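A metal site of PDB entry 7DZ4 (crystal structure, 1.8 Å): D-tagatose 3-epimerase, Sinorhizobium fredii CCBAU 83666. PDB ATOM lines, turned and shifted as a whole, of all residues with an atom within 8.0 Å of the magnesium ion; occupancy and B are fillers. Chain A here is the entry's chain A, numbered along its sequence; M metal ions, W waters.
A ring nitrogen (NE2) of His 205 lies close to a ring nitrogen (NE2) of His 177 (3.5 Å).
The side-chain carboxylate of Asp 179 is in hydrogen-bond range of the backbone NH of Tyr 181 (2.8 Å).
The backbone NH (N) of Thr 180 is in hydrogen-bond range of the backbone carbonyl oxygen (O) of His 205, at 2.9 Å.
O of Gly 103 sits at hydrogen-bond distance from N of Glu 146 (2.9 Å).
OE1 of Glu 38 sits at hydrogen-bond distance from NE2 of His 205 (2.7 Å).
The backbone carbonyl oxygen (O) of Glu 240 is in hydrogen-bond range of the side-chain hydroxyl (OG) of Ser 207 (3.3 Å).
The side-chain carboxylate (OD1) of Asp 179 is in salt-bridge range of the guanidinium group (NH1) of Arg 211.
The backbone NH of Glu 240 sits at hydrogen-bond distance from the backbone carbonyl oxygen of Leu 206 (3.1 Å).
The magnesium ion is bound by OE2 of Glu 146 (2.0 Å), OD2 of Asp 179 (2.0 Å), water W1 (2.1 Å), ND1 of His 205 (2.2 Å), OE1 of Glu 240 (2.4 Å) and water W2 (2.5 Å).
Water W1 lies within hydrogen-bond range of the guanidinium group of Arg 211 (2.8 Å) and a ring nitrogen (NE2) of His 182 (2.9 Å).
Water W2 lies within hydrogen-bond range of OE2 of Glu 240 and OE1 of Glu 146.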
ATOM      1  N   HIS A   9      21.785  14.041   0.544  1.00  0.00           N
ATOM      2  CA  HIS A   9      22.133  13.945  -0.875  1.00  0.00           C
ATOM      3  C   HIS A   9      21.689  12.578  -1.359  1.00  0.00           C
ATOM      4  O   HIS A   9      22.050  11.572  -0.763  1.00  0.00           O
ATOM      5  CB  HIS A   9      23.637  14.124  -1.058  1.00  0.00           C
ATOM      6  CG  HIS A   9      24.059  14.296  -2.479  1.00  0.00           C
ATOM      7  ND1 HIS A   9      23.730  13.395  -3.466  1.00  0.00           N
ATOM      8  CD2 HIS A   9      24.813  15.247  -3.082  1.00  0.00           C
ATOM      9  CE1 HIS A   9      24.222  13.803  -4.620  1.00  0.00           C
ATOM     10  NE2 HIS A   9      24.896  14.919  -4.411  1.00  0.00           N
ATOM     11  N   GLU A  38      18.649  16.555  -1.692  1.00  0.00           N
ATOM     12  CA  GLU A  38      19.496  17.162  -2.703  1.00  0.00           C
ATOM     13  C   GLU A  38      19.528  16.245  -3.906  1.00  0.00           C
ATOM     14  O   GLU A  38      19.943  15.090  -3.790  1.00  0.00           O
ATOM     15  CB  GLU A  38      20.901  17.429  -2.166  1.00  0.00           C
ATOM     16  CG  GLU A  38      21.840  17.976  -3.219  1.00  0.00           C
ATOM     17  CD  GLU A  38      23.213  18.224  -2.636  1.00  0.00           C
ATOM     18  OE1 GLU A  38      23.311  18.182  -1.395  1.00  0.00           O
ATOM     19  OE2 GLU A  38      24.164  18.441  -3.387  1.00  0.00           O
ATOM     20  N   SER A  66      22.031  19.788  -7.434  1.00  0.00           N
ATOM     21  CA  SER A  66      23.450  20.077  -7.516  1.00  0.00           C
ATOM     22  C   SER A  66      24.064  19.377  -8.725  1.00  0.00           C
ATOM     23  O   SER A  66      23.508  18.407  -9.263  1.00  0.00           O
ATOM     24  CB  SER A  66      24.161  19.655  -6.234  1.00  0.00           C
ATOM     25  OG  SER A  66      23.983  18.271  -6.032  1.00  0.00           O
ATOM     26  N   GLY A 103      26.653  23.194  -5.813  1.00  0.00           N
ATOM     27  CA  GLY A 103      27.674  22.287  -6.222  1.00  0.00           C
ATOM     28  C   GLY A 103      28.871  22.942  -6.868  1.00  0.00           C
ATOM     29  O   GLY A 103      29.157  24.123  -6.647  1.00  0.00           O
ATOM     30  N   VAL A 104      29.537  22.168  -7.688  1.00  0.00           N
ATOM     31  CA  VAL A 104      30.678  22.650  -8.481  1.00  0.00           C
ATOM     32  C   VAL A 104      30.137  23.256  -9.763  1.00  0.00           C
ATOM     33  O   VAL A 104      30.371  22.750 -10.882  1.00  0.00           O
ATOM     34  CB  VAL A 104      31.681  21.512  -8.748  1.00  0.00           C
ATOM     35  CG1 VAL A 104      32.984  22.093  -9.316  1.00  0.00           C
ATOM     36  CG2 VAL A 104      31.951  20.755  -7.457  1.00  0.00           C
ATOM     37  N   GLU A 146      30.093  25.323  -4.127  1.00  0.00           N
ATOM     38  CA  GLU A 146      30.638  24.349  -3.195  1.00  0.00           C
ATOM     39  C   GLU A 146      32.157  24.292  -3.326  1.00  0.00           C
ATOM     40  O   GLU A 146      32.696  23.946  -4.384  1.00  0.00           O
ATOM     41  CB  GLU A 146      30.067  22.945  -3.400  1.00  0.00           C
ATOM     42  CG  GLU A 146      30.651  21.869  -2.437  1.00  0.00           C
ATOM     43  CD  GLU A 146      30.030  20.475  -2.569  1.00  0.00           C
ATOM     44  OE1 GLU A 146      29.270  20.260  -3.559  1.00  0.00           O
ATOM     45  OE2 GLU A 146      30.239  19.614  -1.668  1.00  0.00           O
ATOM     46  N   ALA A 147      32.827  24.645  -2.249  1.00  0.00           N
ATOM     47  CA  ALA A 147      34.262  24.551  -2.170  1.00  0.00           C
ATOM     48  C   ALA A 147      34.623  23.073  -2.079  1.00  0.00           C
ATOM     49  O   ALA A 147      34.069  22.352  -1.245  1.00  0.00           O
ATOM     50  CB  ALA A 147      34.721  25.312  -0.927  1.00  0.00           C
ATOM     51  N   VAL A 148      35.538  22.640  -2.941  1.00  0.00           N
ATOM     52  CA  VAL A 148      35.966  21.235  -2.978  1.00  0.00           C
ATOM     53  C   VAL A 148      37.489  21.152  -2.863  1.00  0.00           C
ATOM     54  O   VAL A 148      38.188  22.137  -3.003  1.00  0.00           O
ATOM     55  CB  VAL A 148      35.510  20.487  -4.248  1.00  0.00           C
ATOM     56  CG1 VAL A 148      33.976  20.470  -4.366  1.00  0.00           C
ATOM     57  CG2 VAL A 148      36.137  21.091  -5.482  1.00  0.00           C
ATOM     58  N   GLU A 152      40.236  17.905  -6.708  1.00  0.00           N
ATOM     59  CA  GLU A 152      39.093  17.831  -7.607  1.00  0.00           C
ATOM     60  C   GLU A 152      39.041  19.015  -8.527  1.00  0.00           C
ATOM     61  O   GLU A 152      38.480  18.925  -9.630  1.00  0.00           O
ATOM     62  CB  GLU A 152      37.820  17.728  -6.786  1.00  0.00           C
ATOM     63  CG  GLU A 152      37.870  16.465  -5.932  1.00  0.00           C
ATOM     64  CD  GLU A 152      36.476  15.984  -5.526  1.00  0.00           C
ATOM     65  OE1 GLU A 152      35.519  16.804  -5.567  1.00  0.00           O
ATOM     66  OE2 GLU A 152      36.365  14.794  -5.150  1.00  0.00           O
ATOM     67  N   HIS A 177      28.575  26.878  -0.070  1.00  0.00           N
ATOM     68  CA  HIS A 177      28.190  25.494   0.200  1.00  0.00           C
ATOM     69  C   HIS A 177      29.497  24.841   0.609  1.00  0.00           C
ATOM     70  O   HIS A 177      30.460  24.883  -0.140  1.00  0.00           O
ATOM     71  CB  HIS A 177      27.546  24.905  -1.068  1.00  0.00           C
ATOM     72  CG  HIS A 177      27.321  23.427  -1.046  1.00  0.00           C
ATOM     73  ND1 HIS A 177      26.516  22.784  -1.980  1.00  0.00           N
ATOM     74  CD2 HIS A 177      27.789  22.456  -0.231  1.00  0.00           C
ATOM     75  CE1 HIS A 177      26.533  21.484  -1.751  1.00  0.00           C
ATOM     76  NE2 HIS A 177      27.267  21.261  -0.674  1.00  0.00           N
ATOM     77  N   LEU A 178      29.602  24.438   1.876  1.00  0.00           N
ATOM     78  CA  LEU A 178      30.791  23.796   2.387  1.00  0.00           C
ATOM     79  C   LEU A 178      30.532  22.303   2.488  1.00  0.00           C
ATOM     80  O   LEU A 178      29.381  21.847   2.466  1.00  0.00           O
ATOM     81  CB  LEU A 178      31.154  24.357   3.776  1.00  0.00           C
ATOM     82  CG  LEU A 178      31.581  25.813   3.794  1.00  0.00           C
ATOM     83  CD1 LEU A 178      31.877  26.355   5.243  1.00  0.00           C
ATOM     84  CD2 LEU A 178      32.799  25.983   2.921  1.00  0.00           C
ATOM     85  N   ASP A 179      31.596  21.545   2.612  1.00  0.00           N
ATOM     86  CA  ASP A 179      31.522  20.094   2.722  1.00  0.00           C
ATOM     87  C   ASP A 179      32.599  19.659   3.697  1.00  0.00           C
ATOM     88  O   ASP A 179      33.781  19.924   3.464  1.00  0.00           O
ATOM     89  CB  ASP A 179      31.680  19.499   1.325  1.00  0.00           C
ATOM     90  CG  ASP A 179      31.642  18.014   1.290  1.00  0.00           C
ATOM     91  OD1 ASP A 179      32.253  17.393   2.149  1.00  0.00           O
ATOM     92  OD2 ASP A 179      31.061  17.463   0.341  1.00  0.00           O
ATOM     93  N   THR A 180      32.198  19.015   4.796  1.00  0.00           N
ATOM     94  CA  THR A 180      33.163  18.696   5.842  1.00  0.00           C
ATOM     95  C   THR A 180      34.272  17.812   5.353  1.00  0.00           C
ATOM     96  O   THR A 180      35.391  17.909   5.836  1.00  0.00           O
ATOM     97  CB  THR A 180      32.441  18.031   7.026  1.00  0.00           C
ATOM     98  OG1 THR A 180      31.737  16.848   6.573  1.00  0.00           O
ATOM     99  CG2 THR A 180      31.474  19.019   7.634  1.00  0.00           C
ATOM    100  N   TYR A 181      34.005  16.964   4.344  1.00  0.00           N
ATOM    101  CA  TYR A 181      35.045  16.112   3.804  1.00  0.00           C
ATOM    102  C   TYR A 181      36.113  16.940   3.100  1.00  0.00           C
ATOM    103  O   TYR A 181      37.311  16.658   3.200  1.00  0.00           O
ATOM    104  CB  TYR A 181      34.404  15.093   2.836  1.00  0.00           C
ATOM    105  CG  TYR A 181      35.368  14.394   1.890  1.00  0.00           C
ATOM    106  CD1 TYR A 181      35.715  14.961   0.669  1.00  0.00           C
ATOM    107  CD2 TYR A 181      35.898  13.160   2.222  1.00  0.00           C
ATOM    108  CE1 TYR A 181      36.554  14.302  -0.210  1.00  0.00           C
ATOM    109  CE2 TYR A 181      36.728  12.499   1.375  1.00  0.00           C
ATOM    110  CZ  TYR A 181      37.066  13.082   0.167  1.00  0.00           C
ATOM    111  OH  TYR A 181      37.876  12.399  -0.652  1.00  0.00           O
ATOM    112  N   HIS A 182      35.697  17.988   2.384  1.00  0.00           N
ATOM    113  CA  HIS A 182      36.705  18.821   1.710  1.00  0.00           C
ATOM    114  C   HIS A 182      37.385  19.738   2.708  1.00  0.00           C
ATOM    115  O   HIS A 182      38.603  19.975   2.618  1.00  0.00           O
ATOM    116  CB  HIS A 182      36.059  19.638   0.613  1.00  0.00           C
ATOM    117  CG  HIS A 182      35.477  18.802  -0.490  1.00  0.00           C
ATOM    118  ND1 HIS A 182      36.222  17.902  -1.227  1.00  0.00           N
ATOM    119  CD2 HIS A 182      34.212  18.716  -0.954  1.00  0.00           C
ATOM    120  CE1 HIS A 182      35.435  17.274  -2.086  1.00  0.00           C
ATOM    121  NE2 HIS A 182      34.212  17.772  -1.963  1.00  0.00           N
ATOM    122  N   TYR A 203      24.527  26.216   3.379  1.00  0.00           N
ATOM    123  CA  TYR A 203      24.365  24.806   3.129  1.00  0.00           C
ATOM    124  C   TYR A 203      25.677  24.115   3.444  1.00  0.00           C
ATOM    125  O   TYR A 203      26.740  24.611   3.106  1.00  0.00           O
ATOM    126  CB  TYR A 203      23.996  24.596   1.652  1.00  0.00           C
ATOM    127  CG  TYR A 203      23.433  23.266   1.315  1.00  0.00           C
ATOM    128  CD1 TYR A 203      22.114  22.961   1.604  1.00  0.00           C
ATOM    129  CD2 TYR A 203      24.192  22.327   0.632  1.00  0.00           C
ATOM    130  CE1 TYR A 203      21.584  21.750   1.255  1.00  0.00           C
ATOM    131  CE2 TYR A 203      23.655  21.106   0.275  1.00  0.00           C
ATOM    132  CZ  TYR A 203      22.347  20.824   0.589  1.00  0.00           C
ATOM    133  OH  TYR A 203      21.792  19.634   0.237  1.00  0.00           O
ATOM    134  N   ILE A 204      25.592  22.962   4.087  1.00  0.00           N
ATOM    135  CA  ILE A 204      26.809  22.215   4.362  1.00  0.00           C
ATOM    136  C   ILE A 204      26.546  20.744   4.184  1.00  0.00           C
ATOM    137  O   ILE A 204      25.532  20.217   4.646  1.00  0.00           O
ATOM    138  CB  ILE A 204      27.336  22.562   5.768  1.00  0.00           C
ATOM    139  CG1 ILE A 204      28.681  21.891   6.036  1.00  0.00           C
ATOM    140  CG2 ILE A 204      26.358  22.178   6.808  1.00  0.00           C
ATOM    141  CD1 ILE A 204      29.468  22.587   7.243  1.00  0.00           C
ATOM    142  N   HIS A 205      27.477  20.084   3.503  1.00  0.00           N
ATOM    143  CA  HIS A 205      27.497  18.635   3.398  1.00  0.00           C
ATOM    144  C   HIS A 205      28.202  18.101   4.628  1.00  0.00           C
ATOM    145  O   HIS A 205      29.359  18.469   4.879  1.00  0.00           O
ATOM    146  CB  HIS A 205      28.273  18.188   2.157  1.00  0.00           C
ATOM    147  CG  HIS A 205      27.453  18.112   0.926  1.00  0.00           C
ATOM    148  ND1 HIS A 205      27.985  17.993  -0.344  1.00  0.00           N
ATOM    149  CD2 HIS A 205      26.109  18.163   0.764  1.00  0.00           C
ATOM    150  CE1 HIS A 205      27.005  17.979  -1.224  1.00  0.00           C
ATOM    151  NE2 HIS A 205      25.855  18.087  -0.581  1.00  0.00           N
ATOM    152  N   LEU A 206      27.486  17.274   5.384  1.00  0.00           N
ATOM    153  CA  LEU A 206      28.040  16.557   6.529  1.00  0.00           C
ATOM    154  C   LEU A 206      28.466  15.194   6.016  1.00  0.00           C
ATOM    155  O   LEU A 206      27.646  14.283   5.797  1.00  0.00           O
ATOM    156  CB  LEU A 206      27.011  16.481   7.657  1.00  0.00           C
ATOM    157  CG  LEU A 206      26.423  17.881   7.930  1.00  0.00           C
ATOM    158  CD1 LEU A 206      25.212  17.663   8.848  1.00  0.00           C
ATOM    159  CD2 LEU A 206      27.450  18.890   8.572  1.00  0.00           C
ATOM    160  N   SER A 207      29.754  15.085   5.770  1.00  0.00           N
ATOM    161  CA  SER A 207      30.349  13.885   5.243  1.00  0.00           C
ATOM    162  C   SER A 207      31.563  13.560   6.077  1.00  0.00           C
ATOM    163  O   SER A 207      32.300  14.451   6.510  1.00  0.00           O
ATOM    164  CB  SER A 207      30.716  14.103   3.757  1.00  0.00           C
ATOM    165  OG  SER A 207      31.433  13.012   3.220  1.00  0.00           O
ATOM    166  N   ARG A 211      34.377   9.544   3.264  1.00  0.00           N
ATOM    167  CA  ARG A 211      33.097   9.463   2.572  1.00  0.00           C
ATOM    168  C   ARG A 211      32.202   8.350   3.094  1.00  0.00           C
ATOM    169  O   ARG A 211      31.176   8.065   2.478  1.00  0.00           O
ATOM    170  CB  ARG A 211      33.267   9.345   1.058  1.00  0.00           C
ATOM    171  CG  ARG A 211      33.842  10.613   0.401  1.00  0.00           C
ATOM    172  CD  ARG A 211      33.007  11.819   0.651  1.00  0.00           C
ATOM    173  NE  ARG A 211      33.219  12.865  -0.364  1.00  0.00           N
ATOM    174  CZ  ARG A 211      32.584  14.028  -0.364  1.00  0.00           C
ATOM    175  NH1 ARG A 211      31.730  14.292   0.618  1.00  0.00           N
ATOM    176  NH2 ARG A 211      32.792  14.905  -1.373  1.00  0.00           N
ATOM    177  N   ALA A 238      22.979  18.725   5.260  1.00  0.00           N
ATOM    178  CA  ALA A 238      22.782  17.664   4.282  1.00  0.00           C
ATOM    179  C   ALA A 238      23.825  16.575   4.470  1.00  0.00           C
ATOM    180  O   ALA A 238      25.011  16.815   4.238  1.00  0.00           O
ATOM    181  CB  ALA A 238      22.897  18.215   2.874  1.00  0.00           C
ATOM    182  N   GLU A 240      26.002  13.530   3.298  1.00  0.00           N
ATOM    183  CA  GLU A 240      26.515  12.994   2.051  1.00  0.00           C
ATOM    184  C   GLU A 240      27.413  11.807   2.362  1.00  0.00           C
ATOM    185  O   GLU A 240      28.349  11.926   3.154  1.00  0.00           O
ATOM    186  CB  GLU A 240      27.290  14.054   1.272  1.00  0.00           C
ATOM    187  CG  GLU A 240      27.904  13.522  -0.033  1.00  0.00           C
ATOM    188  CD  GLU A 240      28.376  14.664  -0.980  1.00  0.00           C
ATOM    189  OE1 GLU A 240      29.258  15.465  -0.588  1.00  0.00           O
ATOM    190  OE2 GLU A 240      27.870  14.774  -2.114  1.00  0.00           O
ATOM    191  N   PHE A 242      29.240   8.303   0.150  1.00  0.00           N
ATOM    192  CA  PHE A 242      29.392   7.704  -1.179  1.00  0.00           C
ATOM    193  C   PHE A 242      29.006   6.220  -1.199  1.00  0.00           C
ATOM    194  O   PHE A 242      29.194   5.544  -2.220  1.00  0.00           O
ATOM    195  CB  PHE A 242      30.819   7.905  -1.699  1.00  0.00           C
ATOM    196  CG  PHE A 242      31.104   9.325  -2.162  1.00  0.00           C
ATOM    197  CD1 PHE A 242      30.128  10.320  -2.105  1.00  0.00           C
ATOM    198  CD2 PHE A 242      32.357   9.666  -2.636  1.00  0.00           C
ATOM    199  CE1 PHE A 242      30.400  11.628  -2.522  1.00  0.00           C
ATOM    200  CE2 PHE A 242      32.631  10.970  -3.039  1.00  0.00           C
ATOM    201  CZ  PHE A 242      31.635  11.943  -2.976  1.00  0.00           C
ATOM    202  N   LEU A 253      35.011   9.962  -8.756  1.00  0.00           N
ATOM    203  CA  LEU A 253      35.280  10.614  -7.472  1.00  0.00           C
ATOM    204  C   LEU A 253      36.380   9.931  -6.661  1.00  0.00           C
ATOM    205  O   LEU A 253      36.529  10.154  -5.447  1.00  0.00           O
ATOM    206  CB  LEU A 253      34.000  10.642  -6.643  1.00  0.00           C
ATOM    207  CG  LEU A 253      33.039  11.701  -7.179  1.00  0.00           C
ATOM    208  CD1 LEU A 253      31.605  11.276  -6.907  1.00  0.00           C
ATOM    209  CD2 LEU A 253      33.368  13.023  -6.510  1.00  0.00           C
HETATM  210 MG    MG M   1      29.895  17.681  -1.281  1.00  0.00          MG
HETATM  211  O   HOH W   1      31.444  17.069  -2.553  1.00  0.00           O
HETATM  212  O   HOH W   2      29.260  17.028  -3.610  1.00  0.00           O
